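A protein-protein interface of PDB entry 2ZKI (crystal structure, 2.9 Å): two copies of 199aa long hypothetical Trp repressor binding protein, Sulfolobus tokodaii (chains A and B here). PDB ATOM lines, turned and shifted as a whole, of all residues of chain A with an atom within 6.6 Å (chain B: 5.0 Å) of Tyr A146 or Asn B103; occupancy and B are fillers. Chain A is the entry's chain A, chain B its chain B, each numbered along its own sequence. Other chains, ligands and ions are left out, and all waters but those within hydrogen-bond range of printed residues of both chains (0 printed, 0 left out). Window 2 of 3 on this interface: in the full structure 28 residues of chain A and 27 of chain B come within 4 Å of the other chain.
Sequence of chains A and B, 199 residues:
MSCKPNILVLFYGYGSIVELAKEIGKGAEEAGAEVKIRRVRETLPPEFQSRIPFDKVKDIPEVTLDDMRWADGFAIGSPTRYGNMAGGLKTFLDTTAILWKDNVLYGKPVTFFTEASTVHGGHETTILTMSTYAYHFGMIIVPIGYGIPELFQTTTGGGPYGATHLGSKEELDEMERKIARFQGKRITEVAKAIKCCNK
Trp B100 touches Tyr A146 (CZ2 to CE1, 3.6 Å). Tyr A146 touches Asn B103. Tyr A146 touches Tyr B106 (N to CE1, 3.9 Å). Tyr A146 touches His B136. Gly A147 touches Tyr B106 (N to CE1, 3.6 Å). Phe A152 touches Trp B100. His B136 touches Pro A160 (CA to CB, 3.8 Å). Tyr B106 touches Phe A182.
The backbone carbonyl oxygen (O) of Pro A160 sits at hydrogen-bond distance from the backbone NH (N) of Gly A145, at 3.1 Å. O of Trp B100 lies close to OD1 of Asn B103 (3.5 Å). The backbone NH (N) of Ile A144 sits at hydrogen-bond distance from the backbone carbonyl oxygen (O) of Pro A160. NE1 of Trp B100 is in hydrogen-bond range of O of His B136.
O of Ile A144 lies within hydrogen-bond range of OH of Tyr B106 (2.5 Å).
No position is printed for both chains.
Of the 9 printed residues of chain B, 4 touch a printed residue of chain A. Printed residues of chain B that touch a printed residue of chain A: Trp B100, Asn B103, Tyr B106 and His B136. Hydrophobic or aromatic side chains of chain B within 4 Å of the printed part of chain A: Trp B100, Tyr B106 and His B136.
Of the printed residues of chain B, Ile A144 touches Tyr B106 (2.5 Å). Of chain B, only Trp B100, Asn B103, Tyr B106 and His B136 come within 4 Å of Tyr A146. Printed residues of chain A within 4 Å of Trp B100: Tyr A146 and Phe A152. Asn B103 touches just one residue of chain A: Tyr A146. The nearest printed residue of chain B that does not touch Tyr A146 is Lys B101 (6.1 Å). The nearest residue of chain A that does not touch Asn B103 is Gly A147 (4.6 Å). The nearest printed residue of chain A that does not touch His B136 is Gly A145 (4.3 Å).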
ATOM      1  N   ILE A 144      -2.244   9.222  13.486  1.00  0.00           N
ATOM      2  CA  ILE A 144      -2.345  10.569  12.917  1.00  0.00           C
ATOM      3  C   ILE A 144      -3.453  11.404  13.560  1.00  0.00           C
ATOM      4  O   ILE A 144      -3.375  12.635  13.579  1.00  0.00           O
ATOM      5  CB  ILE A 144      -2.479  10.572  11.376  1.00  0.00           C
ATOM      6  CG1 ILE A 144      -3.551   9.585  10.904  1.00  0.00           C
ATOM      7  CG2 ILE A 144      -1.134  10.275  10.745  1.00  0.00           C
ATOM      8  CD1 ILE A 144      -3.851   9.677   9.425  1.00  0.00           C
ATOM      9  N   GLY A 145      -4.471  10.727  14.089  1.00  0.00           N
ATOM     10  CA  GLY A 145      -5.557  11.386  14.801  1.00  0.00           C
ATOM     11  C   GLY A 145      -6.325  12.331  13.906  1.00  0.00           C
ATOM     12  O   GLY A 145      -6.825  11.932  12.855  1.00  0.00           O
ATOM     13  N   TYR A 146      -6.416  13.588  14.328  1.00  0.00           N
ATOM     14  CA  TYR A 146      -7.076  14.622  13.540  1.00  0.00           C
ATOM     15  C   TYR A 146      -6.212  15.878  13.489  1.00  0.00           C
ATOM     16  O   TYR A 146      -6.662  16.976  13.827  1.00  0.00           O
ATOM     17  CB  TYR A 146      -8.474  14.921  14.092  1.00  0.00           C
ATOM     18  CG  TYR A 146      -9.448  13.763  13.991  1.00  0.00           C
ATOM     19  CD1 TYR A 146      -9.657  12.906  15.071  1.00  0.00           C
ATOM     20  CD2 TYR A 146     -10.161  13.525  12.814  1.00  0.00           C
ATOM     21  CE1 TYR A 146     -10.550  11.841  14.986  1.00  0.00           C
ATOM     22  CE2 TYR A 146     -11.059  12.461  12.719  1.00  0.00           C
ATOM     23  CZ  TYR A 146     -11.246  11.627  13.810  1.00  0.00           C
ATOM     24  OH  TYR A 146     -12.125  10.576  13.725  1.00  0.00           O
ATOM     25  N   GLY A 147      -4.964  15.695  13.062  1.00  0.00           N
ATOM     26  CA  GLY A 147      -3.990  16.783  12.953  1.00  0.00           C
ATOM     27  C   GLY A 147      -4.360  17.812  11.901  1.00  0.00           C
ATOM     28  O   GLY A 147      -4.405  19.009  12.187  1.00  0.00           O
ATOM     29  N   ILE A 148      -4.624  17.344  10.684  1.00  0.00           N
ATOM     30  CA  ILE A 148      -5.044  18.224   9.591  1.00  0.00           C
ATOM     31  C   ILE A 148      -6.573  18.236   9.411  1.00  0.00           C
ATOM     32  O   ILE A 148      -7.237  17.230   9.681  1.00  0.00           O
ATOM     33  CB  ILE A 148      -4.319  17.893   8.252  1.00  0.00           C
ATOM     34  CG1 ILE A 148      -4.492  16.414   7.872  1.00  0.00           C
ATOM     35  CG2 ILE A 148      -2.847  18.290   8.339  1.00  0.00           C
ATOM     36  CD1 ILE A 148      -4.218  16.110   6.408  1.00  0.00           C
ATOM     37  N   PRO A 149      -7.134  19.376   8.957  1.00  0.00           N
ATOM     38  CA  PRO A 149      -8.586  19.507   8.794  1.00  0.00           C
ATOM     39  C   PRO A 149      -9.204  18.526   7.787  1.00  0.00           C
ATOM     40  O   PRO A 149     -10.416  18.297   7.823  1.00  0.00           O
ATOM     41  CB  PRO A 149      -8.756  20.950   8.305  1.00  0.00           C
ATOM     42  CG  PRO A 149      -7.433  21.320   7.722  1.00  0.00           C
ATOM     43  CD  PRO A 149      -6.433  20.617   8.579  1.00  0.00           C
ATOM     44  N   LEU A 151      -8.810  15.369   7.750  1.00  0.00           N
ATOM     45  CA  LEU A 151      -9.180  14.152   8.480  1.00  0.00           C
ATOM     46  C   LEU A 151     -10.608  14.201   9.025  1.00  0.00           C
ATOM     47  O   LEU A 151     -11.249  13.159   9.198  1.00  0.00           O
ATOM     48  CB  LEU A 151      -8.176  13.861   9.601  1.00  0.00           C
ATOM     49  CG  LEU A 151      -6.873  13.177   9.169  1.00  0.00           C
ATOM     50  CD1 LEU A 151      -5.767  13.414  10.184  1.00  0.00           C
ATOM     51  CD2 LEU A 151      -7.080  11.687   8.936  1.00  0.00           C
ATOM     52  N   PHE A 152     -11.093  15.411   9.296  1.00  0.00           N
ATOM     53  CA  PHE A 152     -12.500  15.629   9.614  1.00  0.00           C
ATOM     54  C   PHE A 152     -13.342  15.537   8.338  1.00  0.00           C
ATOM     55  O   PHE A 152     -14.429  14.958   8.342  1.00  0.00           O
ATOM     56  CB  PHE A 152     -12.707  17.009  10.246  1.00  0.00           C
ATOM     57  CG  PHE A 152     -12.038  17.191  11.585  1.00  0.00           C
ATOM     58  CD1 PHE A 152     -12.633  16.712  12.751  1.00  0.00           C
ATOM     59  CD2 PHE A 152     -10.829  17.880  11.684  1.00  0.00           C
ATOM     60  CE1 PHE A 152     -12.023  16.895  13.996  1.00  0.00           C
ATOM     61  CE2 PHE A 152     -10.211  18.071  12.926  1.00  0.00           C
ATOM     62  CZ  PHE A 152     -10.812  17.578  14.082  1.00  0.00           C
ATOM     63  N   GLY A 159      -8.317   8.315   8.263  1.00  0.00           N
ATOM     64  CA  GLY A 159      -8.921   8.375   9.590  1.00  0.00           C
ATOM     65  C   GLY A 159      -7.870   8.479  10.677  1.00  0.00           C
ATOM     66  O   GLY A 159      -6.679   8.528  10.379  1.00  0.00           O
ATOM     67  N   PRO A 160      -8.302   8.504  11.951  1.00  0.00           N
ATOM     68  CA  PRO A 160      -7.382   8.685  13.080  1.00  0.00           C
ATOM     69  C   PRO A 160      -6.383   7.540  13.258  1.00  0.00           C
ATOM     70  O   PRO A 160      -5.273   7.758  13.746  1.00  0.00           O
ATOM     71  CB  PRO A 160      -8.319   8.776  14.291  1.00  0.00           C
ATOM     72  CG  PRO A 160      -9.575   8.115  13.862  1.00  0.00           C
ATOM     73  CD  PRO A 160      -9.701   8.364  12.394  1.00  0.00           C
ATOM     74  N   PHE A 182       0.656  13.603   5.271  1.00  0.00           N
ATOM     75  CA  PHE A 182       0.636  14.023   6.667  1.00  0.00           C
ATOM     76  C   PHE A 182       1.154  12.930   7.601  1.00  0.00           C
ATOM     77  O   PHE A 182       1.861  13.221   8.567  1.00  0.00           O
ATOM     78  CB  PHE A 182      -0.765  14.486   7.087  1.00  0.00           C
ATOM     79  CG  PHE A 182      -0.876  14.830   8.548  1.00  0.00           C
ATOM     80  CD1 PHE A 182      -0.161  15.897   9.084  1.00  0.00           C
ATOM     81  CD2 PHE A 182      -1.690  14.077   9.393  1.00  0.00           C
ATOM     82  CE1 PHE A 182      -0.254  16.214  10.435  1.00  0.00           C
ATOM     83  CE2 PHE A 182      -1.792  14.386  10.748  1.00  0.00           C
ATOM     84  CZ  PHE A 182      -1.072  15.459  11.268  1.00  0.00           C
ATOM     85  N   LEU B  99     -11.500  18.553  25.281  1.00  0.00           N
ATOM     86  CA  LEU B  99     -10.091  18.600  24.890  1.00  0.00           C
ATOM     87  C   LEU B  99      -9.846  18.067  23.480  1.00  0.00           C
ATOM     88  O   LEU B  99      -8.774  18.278  22.912  1.00  0.00           O
ATOM     89  CB  LEU B  99      -9.234  17.812  25.888  1.00  0.00           C
ATOM     90  CG  LEU B  99      -9.382  18.101  27.385  1.00  0.00           C
ATOM     91  CD1 LEU B  99      -8.727  16.996  28.206  1.00  0.00           C
ATOM     92  CD2 LEU B  99      -8.807  19.462  27.752  1.00  0.00           C
ATOM     93  N   TRP B 100     -10.842  17.384  22.920  1.00  0.00           N
ATOM     94  CA  TRP B 100     -10.684  16.664  21.657  1.00  0.00           C
ATOM     95  C   TRP B 100     -10.569  17.575  20.437  1.00  0.00           C
ATOM     96  O   TRP B 100      -9.577  17.514  19.707  1.00  0.00           O
ATOM     97  CB  TRP B 100     -11.821  15.654  21.466  1.00  0.00           C
ATOM     98  CG  TRP B 100     -11.740  14.893  20.173  1.00  0.00           C
ATOM     99  CD1 TRP B 100     -10.874  13.880  19.869  1.00  0.00           C
ATOM    100  CD2 TRP B 100     -12.555  15.086  19.010  1.00  0.00           C
ATOM    101  NE1 TRP B 100     -11.098  13.431  18.590  1.00  0.00           N
ATOM    102  CE2 TRP B 100     -12.125  14.152  18.039  1.00  0.00           C
ATOM    103  CE3 TRP B 100     -13.607  15.956  18.692  1.00  0.00           C
ATOM    104  CZ2 TRP B 100     -12.713  14.061  16.771  1.00  0.00           C
ATOM    105  CZ3 TRP B 100     -14.192  15.866  17.430  1.00  0.00           C
ATOM    106  CH2 TRP B 100     -13.741  14.924  16.486  1.00  0.00           C
ATOM    107  N   LYS B 101     -11.577  18.418  20.225  1.00  0.00           N
ATOM    108  CA  LYS B 101     -11.667  19.227  19.006  1.00  0.00           C
ATOM    109  C   LYS B 101     -10.464  20.149  18.807  1.00  0.00           C
ATOM    110  O   LYS B 101      -9.980  20.309  17.684  1.00  0.00           O
ATOM    111  CB  LYS B 101     -12.981  20.025  18.974  1.00  0.00           C
ATOM    112  CG  LYS B 101     -13.273  20.721  17.634  1.00  0.00           C
ATOM    113  CD  LYS B 101     -13.751  19.757  16.541  1.00  0.00           C
ATOM    114  CE  LYS B 101     -15.265  19.565  16.583  1.00  0.00           C
ATOM    115  NZ  LYS B 101     -15.756  18.805  15.401  1.00  0.00           N
ATOM    116  N   ASP B 102      -9.983  20.738  19.901  1.00  0.00           N
ATOM    117  CA  ASP B 102      -8.868  21.688  19.853  1.00  0.00           C
ATOM    118  C   ASP B 102      -7.493  21.045  20.052  1.00  0.00           C
ATOM    119  O   ASP B 102      -6.503  21.750  20.257  1.00  0.00           O
ATOM    120  CB  ASP B 102      -9.079  22.827  20.857  1.00  0.00           C
ATOM    121  CG  ASP B 102      -9.231  22.336  22.289  1.00  0.00           C
ATOM    122  OD1 ASP B 102      -9.020  23.149  23.212  1.00  0.00           O
ATOM    123  OD2 ASP B 102      -9.567  21.149  22.498  1.00  0.00           O
ATOM    124  N   ASN B 103      -7.446  19.714  19.990  1.00  0.00           N
ATOM    125  CA  ASN B 103      -6.192  18.947  20.002  1.00  0.00           C
ATOM    126  C   ASN B 103      -5.240  19.253  21.169  1.00  0.00           C
ATOM    127  O   ASN B 103      -4.030  19.397  20.968  1.00  0.00           O
ATOM    128  CB  ASN B 103      -5.452  19.090  18.656  1.00  0.00           C
ATOM    129  CG  ASN B 103      -6.261  18.570  17.471  1.00  0.00           C
ATOM    130  OD1 ASN B 103      -6.848  17.486  17.522  1.00  0.00           O
ATOM    131  ND2 ASN B 103      -6.278  19.341  16.388  1.00  0.00           N
ATOM    132  N   VAL B 104      -5.788  19.348  22.378  1.00  0.00           N
ATOM    133  CA  VAL B 104      -4.981  19.591  23.579  1.00  0.00           C
ATOM    134  C   VAL B 104      -3.981  18.455  23.824  1.00  0.00           C
ATOM    135  O   VAL B 104      -2.801  18.703  24.077  1.00  0.00           O
ATOM    136  CB  VAL B 104      -5.866  19.787  24.847  1.00  0.00           C
ATOM    137  CG1 VAL B 104      -5.023  20.216  26.042  1.00  0.00           C
ATOM    138  CG2 VAL B 104      -6.951  20.809  24.593  1.00  0.00           C
ATOM    139  N   LEU B 105      -4.460  17.217  23.734  1.00  0.00           N
ATOM    140  CA  LEU B 105      -3.649  16.040  24.044  1.00  0.00           C
ATOM    141  C   LEU B 105      -2.830  15.515  22.856  1.00  0.00           C
ATOM    142  O   LEU B 105      -2.098  14.530  22.987  1.00  0.00           O
ATOM    143  CB  LEU B 105      -4.532  14.922  24.618  1.00  0.00           C
ATOM    144  CG  LEU B 105      -5.456  15.226  25.803  1.00  0.00           C
ATOM    145  CD1 LEU B 105      -6.308  14.013  26.130  1.00  0.00           C
ATOM    146  CD2 LEU B 105      -4.676  15.673  27.030  1.00  0.00           C
ATOM    147  N   TYR B 106      -2.945  16.181  21.709  1.00  0.00           N
ATOM    148  CA  TYR B 106      -2.293  15.730  20.484  1.00  0.00           C
ATOM    149  C   TYR B 106      -0.784  15.579  20.645  1.00  0.00           C
ATOM    150  O   TYR B 106      -0.111  16.474  21.157  1.00  0.00           O
ATOM    151  CB  TYR B 106      -2.603  16.678  19.323  1.00  0.00           C
ATOM    152  CG  TYR B 106      -2.349  16.069  17.960  1.00  0.00           C
ATOM    153  CD1 TYR B 106      -3.376  15.448  17.256  1.00  0.00           C
ATOM    154  CD2 TYR B 106      -1.080  16.103  17.382  1.00  0.00           C
ATOM    155  CE1 TYR B 106      -3.150  14.882  16.008  1.00  0.00           C
ATOM    156  CE2 TYR B 106      -0.842  15.538  16.135  1.00  0.00           C
ATOM    157  CZ  TYR B 106      -1.883  14.930  15.455  1.00  0.00           C
ATOM    158  OH  TYR B 106      -1.659  14.373  14.220  1.00  0.00           O
ATOM    159  N   HIS B 136      -7.705   8.252  18.388  1.00  0.00           N
ATOM    160  CA  HIS B 136      -8.647   9.331  18.083  1.00  0.00           C
ATOM    161  C   HIS B 136      -8.143  10.692  18.538  1.00  0.00           C
ATOM    162  O   HIS B 136      -8.493  11.715  17.949  1.00  0.00           O
ATOM    163  CB  HIS B 136     -10.013   9.045  18.706  1.00  0.00           C
ATOM    164  CG  HIS B 136     -10.715   7.874  18.098  1.00  0.00           C
ATOM    165  ND1 HIS B 136     -11.733   8.012  17.180  1.00  0.00           N
ATOM    166  CD2 HIS B 136     -10.537   6.543  18.266  1.00  0.00           C
ATOM    167  CE1 HIS B 136     -12.158   6.815  16.814  1.00  0.00           C
ATOM    168  NE2 HIS B 136     -11.450   5.907  17.461  1.00  0.00           N
